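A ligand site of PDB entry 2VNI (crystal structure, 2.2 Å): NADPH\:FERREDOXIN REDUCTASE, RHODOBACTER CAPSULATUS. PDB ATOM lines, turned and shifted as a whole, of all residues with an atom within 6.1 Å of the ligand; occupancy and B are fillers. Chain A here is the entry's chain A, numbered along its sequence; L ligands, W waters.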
ATOM      1  N   THR A 128      11.709  26.892  -6.738  1.00  0.00           N
ATOM      2  CA  THR A 128      11.188  28.247  -6.829  1.00  0.00           C
ATOM      3  C   THR A 128      10.790  28.675  -5.427  1.00  0.00           C
ATOM      4  O   THR A 128      10.404  27.845  -4.606  1.00  0.00           O
ATOM      5  CB  THR A 128       9.939  28.361  -7.746  1.00  0.00           C
ATOM      6  OG1 THR A 128       8.878  27.551  -7.239  1.00  0.00           O
ATOM      7  CG2 THR A 128      10.278  27.951  -9.156  1.00  0.00           C
ATOM      8  N   GLY A 129      10.904  29.970  -5.145  1.00  0.00           N
ATOM      9  CA  GLY A 129      10.531  30.479  -3.832  1.00  0.00           C
ATOM     10  C   GLY A 129      11.187  29.778  -2.665  1.00  0.00           C
ATOM     11  O   GLY A 129      12.393  29.534  -2.691  1.00  0.00           O
ATOM     12  N   ALA A 156      14.611  29.746  -9.130  1.00  0.00           N
ATOM     13  CA  ALA A 156      13.874  30.817  -9.798  1.00  0.00           C
ATOM     14  C   ALA A 156      12.894  31.522  -8.875  1.00  0.00           C
ATOM     15  O   ALA A 156      12.037  30.886  -8.246  1.00  0.00           O
ATOM     16  CB  ALA A 156      13.121  30.260 -11.018  1.00  0.00           C
ATOM     17  N   CYS A 157      13.030  32.844  -8.799  1.00  0.00           N
ATOM     18  CA  CYS A 157      12.170  33.688  -7.980  1.00  0.00           C
ATOM     19  C   CYS A 157      11.765  34.919  -8.792  1.00  0.00           C
ATOM     20  O   CYS A 157      12.322  35.163  -9.861  1.00  0.00           O
ATOM     21  CB  CYS A 157      12.912  34.139  -6.726  1.00  0.00           C
ATOM     22  SG  CYS A 157      13.355  32.834  -5.571  1.00  0.00           S
ATOM     23  N   ARG A 158      10.792  35.682  -8.305  1.00  0.00           N
ATOM     24  CA  ARG A 158      10.352  36.880  -9.005  1.00  0.00           C
ATOM     25  C   ARG A 158      11.401  38.009  -8.938  1.00  0.00           C
ATOM     26  O   ARG A 158      11.666  38.667  -9.938  1.00  0.00           O
ATOM     27  CB  ARG A 158       9.053  37.426  -8.406  1.00  0.00           C
ATOM     28  CG  ARG A 158       7.812  36.585  -8.600  1.00  0.00           C
ATOM     29  CD  ARG A 158       6.574  37.465  -8.363  1.00  0.00           C
ATOM     30  NE  ARG A 158       5.398  36.707  -7.958  1.00  0.00           N
ATOM     31  CZ  ARG A 158       5.163  36.275  -6.717  1.00  0.00           C
ATOM     32  NH1 ARG A 158       6.051  36.502  -5.750  1.00  0.00           N
ATOM     33  NH2 ARG A 158       4.058  35.597  -6.448  1.00  0.00           N
ATOM     34  N   GLU A 162      14.730  37.902  -3.237  1.00  0.00           N
ATOM     35  CA  GLU A 162      14.270  36.580  -2.823  1.00  0.00           C
ATOM     36  C   GLU A 162      15.299  35.482  -3.084  1.00  0.00           C
ATOM     37  O   GLU A 162      15.138  34.355  -2.629  1.00  0.00           O
ATOM     38  CB  GLU A 162      12.957  36.239  -3.535  1.00  0.00           C
ATOM     39  CG  GLU A 162      11.978  37.404  -3.541  1.00  0.00           C
ATOM     40  CD  GLU A 162      10.632  37.031  -4.111  1.00  0.00           C
ATOM     41  OE1 GLU A 162       9.833  36.392  -3.384  1.00  0.00           O
ATOM     42  OE2 GLU A 162      10.367  37.378  -5.271  1.00  0.00           O
ATOM     43  N   THR A 192      17.893  32.520 -11.222  1.00  0.00           N
ATOM     44  CA  THR A 192      17.245  33.350 -12.223  1.00  0.00           C
ATOM     45  C   THR A 192      16.053  34.076 -11.624  1.00  0.00           C
ATOM     46  O   THR A 192      15.492  33.637 -10.630  1.00  0.00           O
ATOM     47  CB  THR A 192      16.759  32.541 -13.455  1.00  0.00           C
ATOM     48  OG1 THR A 192      15.740  31.625 -13.047  1.00  0.00           O
ATOM     49  CG2 THR A 192      17.904  31.786 -14.084  1.00  0.00           C
ATOM     50  N   THR A 193      15.687  35.194 -12.235  1.00  0.00           N
ATOM     51  CA  THR A 193      14.546  35.972 -11.787  1.00  0.00           C
ATOM     52  C   THR A 193      13.573  35.976 -12.959  1.00  0.00           C
ATOM     53  O   THR A 193      13.970  35.705 -14.092  1.00  0.00           O
ATOM     54  CB  THR A 193      14.940  37.441 -11.457  1.00  0.00           C
ATOM     55  OG1 THR A 193      15.587  38.023 -12.592  1.00  0.00           O
ATOM     56  CG2 THR A 193      15.880  37.479 -10.254  1.00  0.00           C
ATOM     57  N   THR A 194      12.302  36.253 -12.720  1.00  0.00           N
ATOM     58  CA  THR A 194      11.329  36.273 -13.802  1.00  0.00           C
ATOM     59  C   THR A 194      10.639  37.621 -13.941  1.00  0.00           C
ATOM     60  O   THR A 194       9.867  37.843 -14.884  1.00  0.00           O
ATOM     61  CB  THR A 194      10.272  35.159 -13.605  1.00  0.00           C
ATOM     62  OG1 THR A 194       9.737  35.226 -12.277  1.00  0.00           O
ATOM     63  CG2 THR A 194      10.889  33.778 -13.835  1.00  0.00           C
ATOM     64  N   ARG A 195      10.911  38.517 -12.991  1.00  0.00           N
ATOM     65  CA  ARG A 195      10.335  39.864 -13.002  1.00  0.00           C
ATOM     66  C   ARG A 195      11.424  40.937 -13.083  1.00  0.00           C
ATOM     67  O   ARG A 195      11.534  41.637 -14.079  1.00  0.00           O
ATOM     68  CB  ARG A 195       9.501  40.076 -11.732  1.00  0.00           C
ATOM     69  CG  ARG A 195       8.007  39.765 -11.881  1.00  0.00           C
ATOM     70  CD  ARG A 195       7.761  38.333 -12.307  1.00  0.00           C
ATOM     71  NE  ARG A 195       6.373  38.148 -12.748  1.00  0.00           N
ATOM     72  CZ  ARG A 195       5.457  37.450 -12.081  1.00  0.00           C
ATOM     73  NH1 ARG A 195       5.760  36.856 -10.938  1.00  0.00           N
ATOM     74  NH2 ARG A 195       4.234  37.345 -12.573  1.00  0.00           N
ATOM     75  N   GLY A 202      14.295  33.908 -16.588  1.00  0.00           N
ATOM     76  CA  GLY A 202      13.503  32.803 -17.089  1.00  0.00           C
ATOM     77  C   GLY A 202      13.139  31.685 -16.123  1.00  0.00           C
ATOM     78  O   GLY A 202      13.902  31.349 -15.213  1.00  0.00           O
ATOM     79  N   ARG A 203      11.971  31.096 -16.343  1.00  0.00           N
ATOM     80  CA  ARG A 203      11.469  29.979 -15.534  1.00  0.00           C
ATOM     81  C   ARG A 203      12.361  28.750 -15.712  1.00  0.00           C
ATOM     82  O   ARG A 203      13.017  28.604 -16.747  1.00  0.00           O
ATOM     83  CB  ARG A 203      10.041  29.620 -15.956  1.00  0.00           C
ATOM     84  CG  ARG A 203       9.009  30.681 -15.721  1.00  0.00           C
ATOM     85  CD  ARG A 203       7.652  30.187 -16.170  1.00  0.00           C
ATOM     86  NE  ARG A 203       6.568  30.961 -15.581  1.00  0.00           N
ATOM     87  CZ  ARG A 203       5.291  30.570 -15.574  1.00  0.00           C
ATOM     88  NH1 ARG A 203       4.957  29.406 -16.121  1.00  0.00           N
ATOM     89  NH2 ARG A 203       4.368  31.326 -14.993  1.00  0.00           N
ATOM     90  N   ILE A 204      12.371  27.873 -14.717  1.00  0.00           N
ATOM     91  CA  ILE A 204      13.170  26.645 -14.804  1.00  0.00           C
ATOM     92  C   ILE A 204      12.724  25.856 -16.045  1.00  0.00           C
ATOM     93  O   ILE A 204      13.546  25.437 -16.849  1.00  0.00           O
ATOM     94  CB  ILE A 204      12.987  25.755 -13.555  1.00  0.00           C
ATOM     95  CG1 ILE A 204      13.428  26.499 -12.290  1.00  0.00           C
ATOM     96  CG2 ILE A 204      13.802  24.466 -13.708  1.00  0.00           C
ATOM     97  CD1 ILE A 204      14.894  26.830 -12.249  1.00  0.00           C
ATOM     98  N   THR A 205      11.418  25.662 -16.177  1.00  0.00           N
ATOM     99  CA  THR A 205      10.854  24.926 -17.299  1.00  0.00           C
ATOM    100  C   THR A 205      11.323  25.489 -18.655  1.00  0.00           C
ATOM    101  O   THR A 205      11.867  24.755 -19.481  1.00  0.00           O
ATOM    102  CB  THR A 205       9.315  24.921 -17.253  1.00  0.00           C
ATOM    103  OG1 THR A 205       8.832  26.268 -17.106  1.00  0.00           O
ATOM    104  CG2 THR A 205       8.830  24.092 -16.078  1.00  0.00           C
ATOM    105  N   SER A 234       5.591  25.047  -6.438  1.00  0.00           N
ATOM    106  CA  SER A 234       4.145  24.871  -6.343  1.00  0.00           C
ATOM    107  C   SER A 234       3.758  23.593  -7.068  1.00  0.00           C
ATOM    108  O   SER A 234       4.562  23.028  -7.807  1.00  0.00           O
ATOM    109  CB  SER A 234       3.411  26.039  -6.979  1.00  0.00           C
ATOM    110  OG  SER A 234       3.692  26.122  -8.375  1.00  0.00           O
ATOM    111  N   ALA A 236       1.681  23.308  -9.545  1.00  0.00           N
ATOM    112  CA  ALA A 236       1.687  23.610 -10.978  1.00  0.00           C
ATOM    113  C   ALA A 236       3.104  23.553 -11.527  1.00  0.00           C
ATOM    114  O   ALA A 236       3.341  23.033 -12.599  1.00  0.00           O
ATOM    115  CB  ALA A 236       1.072  24.987 -11.248  1.00  0.00           C
ATOM    116  N   PHE A 237       4.044  24.105 -10.770  1.00  0.00           N
ATOM    117  CA  PHE A 237       5.448  24.111 -11.163  1.00  0.00           C
ATOM    118  C   PHE A 237       5.912  22.670 -11.294  1.00  0.00           C
ATOM    119  O   PHE A 237       6.436  22.268 -12.320  1.00  0.00           O
ATOM    120  CB  PHE A 237       6.286  24.820 -10.091  1.00  0.00           C
ATOM    121  CG  PHE A 237       7.766  24.629 -10.243  1.00  0.00           C
ATOM    122  CD1 PHE A 237       8.479  25.344 -11.194  1.00  0.00           C
ATOM    123  CD2 PHE A 237       8.458  23.753  -9.410  1.00  0.00           C
ATOM    124  CE1 PHE A 237       9.863  25.205 -11.302  1.00  0.00           C
ATOM    125  CE2 PHE A 237       9.829  23.610  -9.507  1.00  0.00           C
ATOM    126  CZ  PHE A 237      10.538  24.331 -10.452  1.00  0.00           C
ATOM    127  N   ASN A 238       5.692  21.900 -10.223  1.00  0.00           N
ATOM    128  CA  ASN A 238       6.070  20.493 -10.184  1.00  0.00           C
ATOM    129  C   ASN A 238       5.564  19.744 -11.409  1.00  0.00           C
ATOM    130  O   ASN A 238       6.307  19.021 -12.039  1.00  0.00           O
ATOM    131  CB  ASN A 238       5.523  19.839  -8.909  1.00  0.00           C
ATOM    132  CG  ASN A 238       6.299  20.226  -7.666  1.00  0.00           C
ATOM    133  OD1 ASN A 238       7.210  21.052  -7.698  1.00  0.00           O
ATOM    134  ND2 ASN A 238       5.943  19.622  -6.532  1.00  0.00           N
ATOM    135  N   ASP A 240       4.532  20.982 -14.423  1.00  0.00           N
ATOM    136  CA  ASP A 240       5.181  21.468 -15.646  1.00  0.00           C
ATOM    137  C   ASP A 240       6.625  21.000 -15.726  1.00  0.00           C
ATOM    138  O   ASP A 240       7.123  20.709 -16.810  1.00  0.00           O
ATOM    139  CB  ASP A 240       5.152  22.996 -15.740  1.00  0.00           C
ATOM    140  CG  ASP A 240       3.743  23.555 -15.870  1.00  0.00           C
ATOM    141  OD1 ASP A 240       2.818  22.810 -16.263  1.00  0.00           O
ATOM    142  OD2 ASP A 240       3.555  24.764 -15.585  1.00  0.00           O
ATOM    143  N   VAL A 241       7.309  20.937 -14.581  1.00  0.00           N
ATOM    144  CA  VAL A 241       8.696  20.504 -14.579  1.00  0.00           C
ATOM    145  C   VAL A 241       8.800  19.003 -14.867  1.00  0.00           C
ATOM    146  O   VAL A 241       9.713  18.583 -15.572  1.00  0.00           O
ATOM    147  CB  VAL A 241       9.412  20.808 -13.234  1.00  0.00           C
ATOM    148  CG1 VAL A 241      10.759  20.104 -13.184  1.00  0.00           C
ATOM    149  CG2 VAL A 241       9.619  22.315 -13.079  1.00  0.00           C
ATOM    150  N   PHE A 267       4.653  24.102  -1.163  1.00  0.00           N
ATOM    151  CA  PHE A 267       3.533  24.593  -0.349  1.00  0.00           C
ATOM    152  C   PHE A 267       2.217  24.118  -0.984  1.00  0.00           C
ATOM    153  O   PHE A 267       2.210  23.635  -2.115  1.00  0.00           O
ATOM    154  CB  PHE A 267       3.558  26.125  -0.265  1.00  0.00           C
ATOM    155  CG  PHE A 267       3.668  26.807  -1.602  1.00  0.00           C
ATOM    156  CD1 PHE A 267       2.567  26.930  -2.439  1.00  0.00           C
ATOM    157  CD2 PHE A 267       4.896  27.321  -2.034  1.00  0.00           C
ATOM    158  CE1 PHE A 267       2.667  27.558  -3.687  1.00  0.00           C
ATOM    159  CE2 PHE A 267       5.018  27.949  -3.283  1.00  0.00           C
ATOM    160  CZ  PHE A 267       3.904  28.067  -4.110  1.00  0.00           C
ATOM    161  N   GLU A 270      -1.956  27.827  -4.708  1.00  0.00           N
ATOM    162  CA  GLU A 270      -1.298  28.560  -5.783  1.00  0.00           C
ATOM    163  C   GLU A 270      -0.133  29.416  -5.322  1.00  0.00           C
ATOM    164  O   GLU A 270       0.719  29.812  -6.120  1.00  0.00           O
ATOM    165  CB  GLU A 270      -2.323  29.409  -6.535  1.00  0.00           C
ATOM    166  CG  GLU A 270      -3.244  28.566  -7.413  1.00  0.00           C
ATOM    167  CD  GLU A 270      -4.146  29.407  -8.307  1.00  0.00           C
ATOM    168  OE1 GLU A 270      -3.618  30.251  -9.072  1.00  0.00           O
ATOM    169  OE2 GLU A 270      -5.380  29.214  -8.249  1.00  0.00           O
ATOM    170  N   GLY A 271      -0.082  29.693  -4.019  1.00  0.00           N
ATOM    171  CA  GLY A 271       1.004  30.488  -3.489  1.00  0.00           C
ATOM    172  C   GLY A 271       0.739  31.967  -3.616  1.00  0.00           C
ATOM    173  O   GLY A 271       0.035  32.403  -4.538  1.00  0.00           O
ATOM    174  N   ILE A 272       1.294  32.750  -2.691  1.00  0.00           N
ATOM    175  CA  ILE A 272       1.095  34.191  -2.714  1.00  0.00           C
ATOM    176  C   ILE A 272       1.957  34.846  -3.805  1.00  0.00           C
ATOM    177  O   ILE A 272       1.367  35.405  -4.759  1.00  0.00           O
ATOM    178  CB  ILE A 272       1.405  34.828  -1.339  1.00  0.00           C
ATOM    179  CG1 ILE A 272       2.707  34.270  -0.752  1.00  0.00           C
ATOM    180  CG2 ILE A 272       0.256  34.564  -0.379  1.00  0.00           C
ATOM    181  CD1 ILE A 272       3.961  35.036  -1.135  1.00  0.00           C
ATOM    182  OXT ILE A 272       3.200  34.755  -3.713  1.00  0.00           O
HETATM  183  P1  LIG L   1       6.652  33.792 -13.294  1.00  0.00           P
HETATM  184  O1  LIG L   1       5.321  33.156 -13.004  1.00  0.00           O
HETATM  185  O2  LIG L   1       6.815  35.067 -12.580  1.00  0.00           O
HETATM  186  O3  LIG L   1       6.921  33.731 -14.755  1.00  0.00           O
HETATM  187  P2  LIG L   1       5.470  32.526  -7.214  1.00  0.00           P
HETATM  188  O4  LIG L   1       4.230  33.044  -7.890  1.00  0.00           O
HETATM  189  O5  LIG L   1       5.160  31.269  -6.428  1.00  0.00           O
HETATM  190  O6  LIG L   1       6.101  33.672  -6.475  1.00  0.00           O
HETATM  191  O7  LIG L   1       6.526  32.154  -8.369  1.00  0.00           O
HETATM  192  C1  LIG L   1       7.854  31.787  -8.061  1.00  0.00           C
HETATM  193  C2  LIG L   1       8.586  31.499  -9.381  1.00  0.00           C
HETATM  194  O8  LIG L   1       8.231  30.327 -10.140  1.00  0.00           O
HETATM  195  C3  LIG L   1       8.492  32.654 -10.384  1.00  0.00           C
HETATM  196  O9  LIG L   1       9.721  32.841 -11.063  1.00  0.00           O
HETATM  197  C4  LIG L   1       7.398  32.186 -11.325  1.00  0.00           C
HETATM  198  O10 LIG L   1       7.616  32.679 -12.647  1.00  0.00           O
HETATM  199  C5  LIG L   1       7.714  30.706 -11.435  1.00  0.00           C
HETATM  200  N1  LIG L   1       6.582  29.817 -11.757  1.00  0.00           N
HETATM  201  C6  LIG L   1       5.334  29.860 -11.213  1.00  0.00           C
HETATM  202  N2  LIG L   1       4.538  28.865 -11.670  1.00  0.00           N
HETATM  203  C7  LIG L   1       5.311  28.194 -12.522  1.00  0.00           C
HETATM  204  C8  LIG L   1       5.127  27.007 -13.360  1.00  0.00           C
HETATM  205  N3  LIG L   1       3.931  26.389 -13.391  1.00  0.00           N
HETATM  206  N4  LIG L   1       6.154  26.585 -14.084  1.00  0.00           N
HETATM  207  C9  LIG L   1       7.330  27.219 -14.079  1.00  0.00           C
HETATM  208  N5  LIG L   1       7.614  28.317 -13.368  1.00  0.00           N
HETATM  209  C10 LIG L   1       6.653  28.775 -12.578  1.00  0.00           C
HETATM  210  O   HOH W   1       3.458  32.729 -10.504  1.00  0.00           O
HETATM  211  O   HOH W   2      10.477  28.542 -12.656  1.00  0.00           O
HETATM  212  O   HOH W   3       7.440  29.731  -4.804  1.00  0.00           O
HETATM  213  O   HOH W   4       2.807  28.372  -9.609  1.00  0.00           O
HETATM  214  O   HOH W   5       6.141  26.388 -17.234  1.00  0.00           O
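O2 of the ligand is in salt-bridge range of NH1 of Arg 195, at 2.6 Å.
The side-chain hydroxyl of Thr 194 sits at hydrogen-bond distance from an oxygen (O9) of the ligand, 2.7 Å away.
A nitrogen (N3) of the ligand is in hydrogen-bond range of the side-chain carboxylate (OD2) of Asp 240 (2.8 Å).
O6 of the ligand lies within salt-bridge range of NH2 of Arg 158.
O1 of the ligand is in salt-bridge range of NH2 of Arg 203.
O of Ala 236 lies close to N3 of the ligand (3.5 Å).
The backbone NH (N) of Arg 195 lies close to the backbone carbonyl oxygen (O) of Arg 158.
The backbone NH of Thr 194 sits at hydrogen-bond distance from the backbone carbonyl oxygen of Cys 157 (3.1 Å).
The guanidinium group of Arg 158 is in salt-bridge range of the chain-end carboxylate of Ile 272 (3.0 Å).
N of Phe 237 sits at hydrogen-bond distance from OG of Ser 234 (3.2 Å).
N of Gly 129 sits at hydrogen-bond distance from O of Ala 156, 3.4 Å away.
N of Gly 129 lies within hydrogen-bond range of SG of Cys 157, 3.8 Å away.
The backbone carbonyl oxygen (O) of Glu 162 lies within hydrogen-bond range of the side-chain sulfur (SG) of Cys 157.
O of Thr 192 sits at hydrogen-bond distance from N of Cys 157 (3.2 Å).
The backbone NH (N) of Phe 237 lies close to a nitrogen (N3) of the ligand (3.5 Å).
Merely in contact with the ligand: Thr 128 (3.3 Å), Thr 205 (3.5 Å), Ala 156 (3.7 Å) and Cys 157 (3.7 Å).
The nearest printed residue that does not touch the ligand is Phe 267 (4.1 Å).
Water W4 bridges the side-chain hydroxyl (OG) of Ser 234 and a nitrogen (N2) of the ligand.
Water W2 bridges the backbone NH of Ile 204 and a nitrogen (N5) of the ligand.
Water W5 lies within hydrogen-bond range of the side-chain hydroxyl (OG1) of Thr 205 (2.7 Å), a nitrogen (N4) of the ligand (3.2 Å), the guanidinium group (NH1) of Arg 203 (3.4 Å) and the side-chain carboxylate (OD2) of Asp 240 (3.5 Å).
Water W3 lies within hydrogen-bond range of O5 of the ligand (3.2 Å) and N of Gly 129 (3.5 Å).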
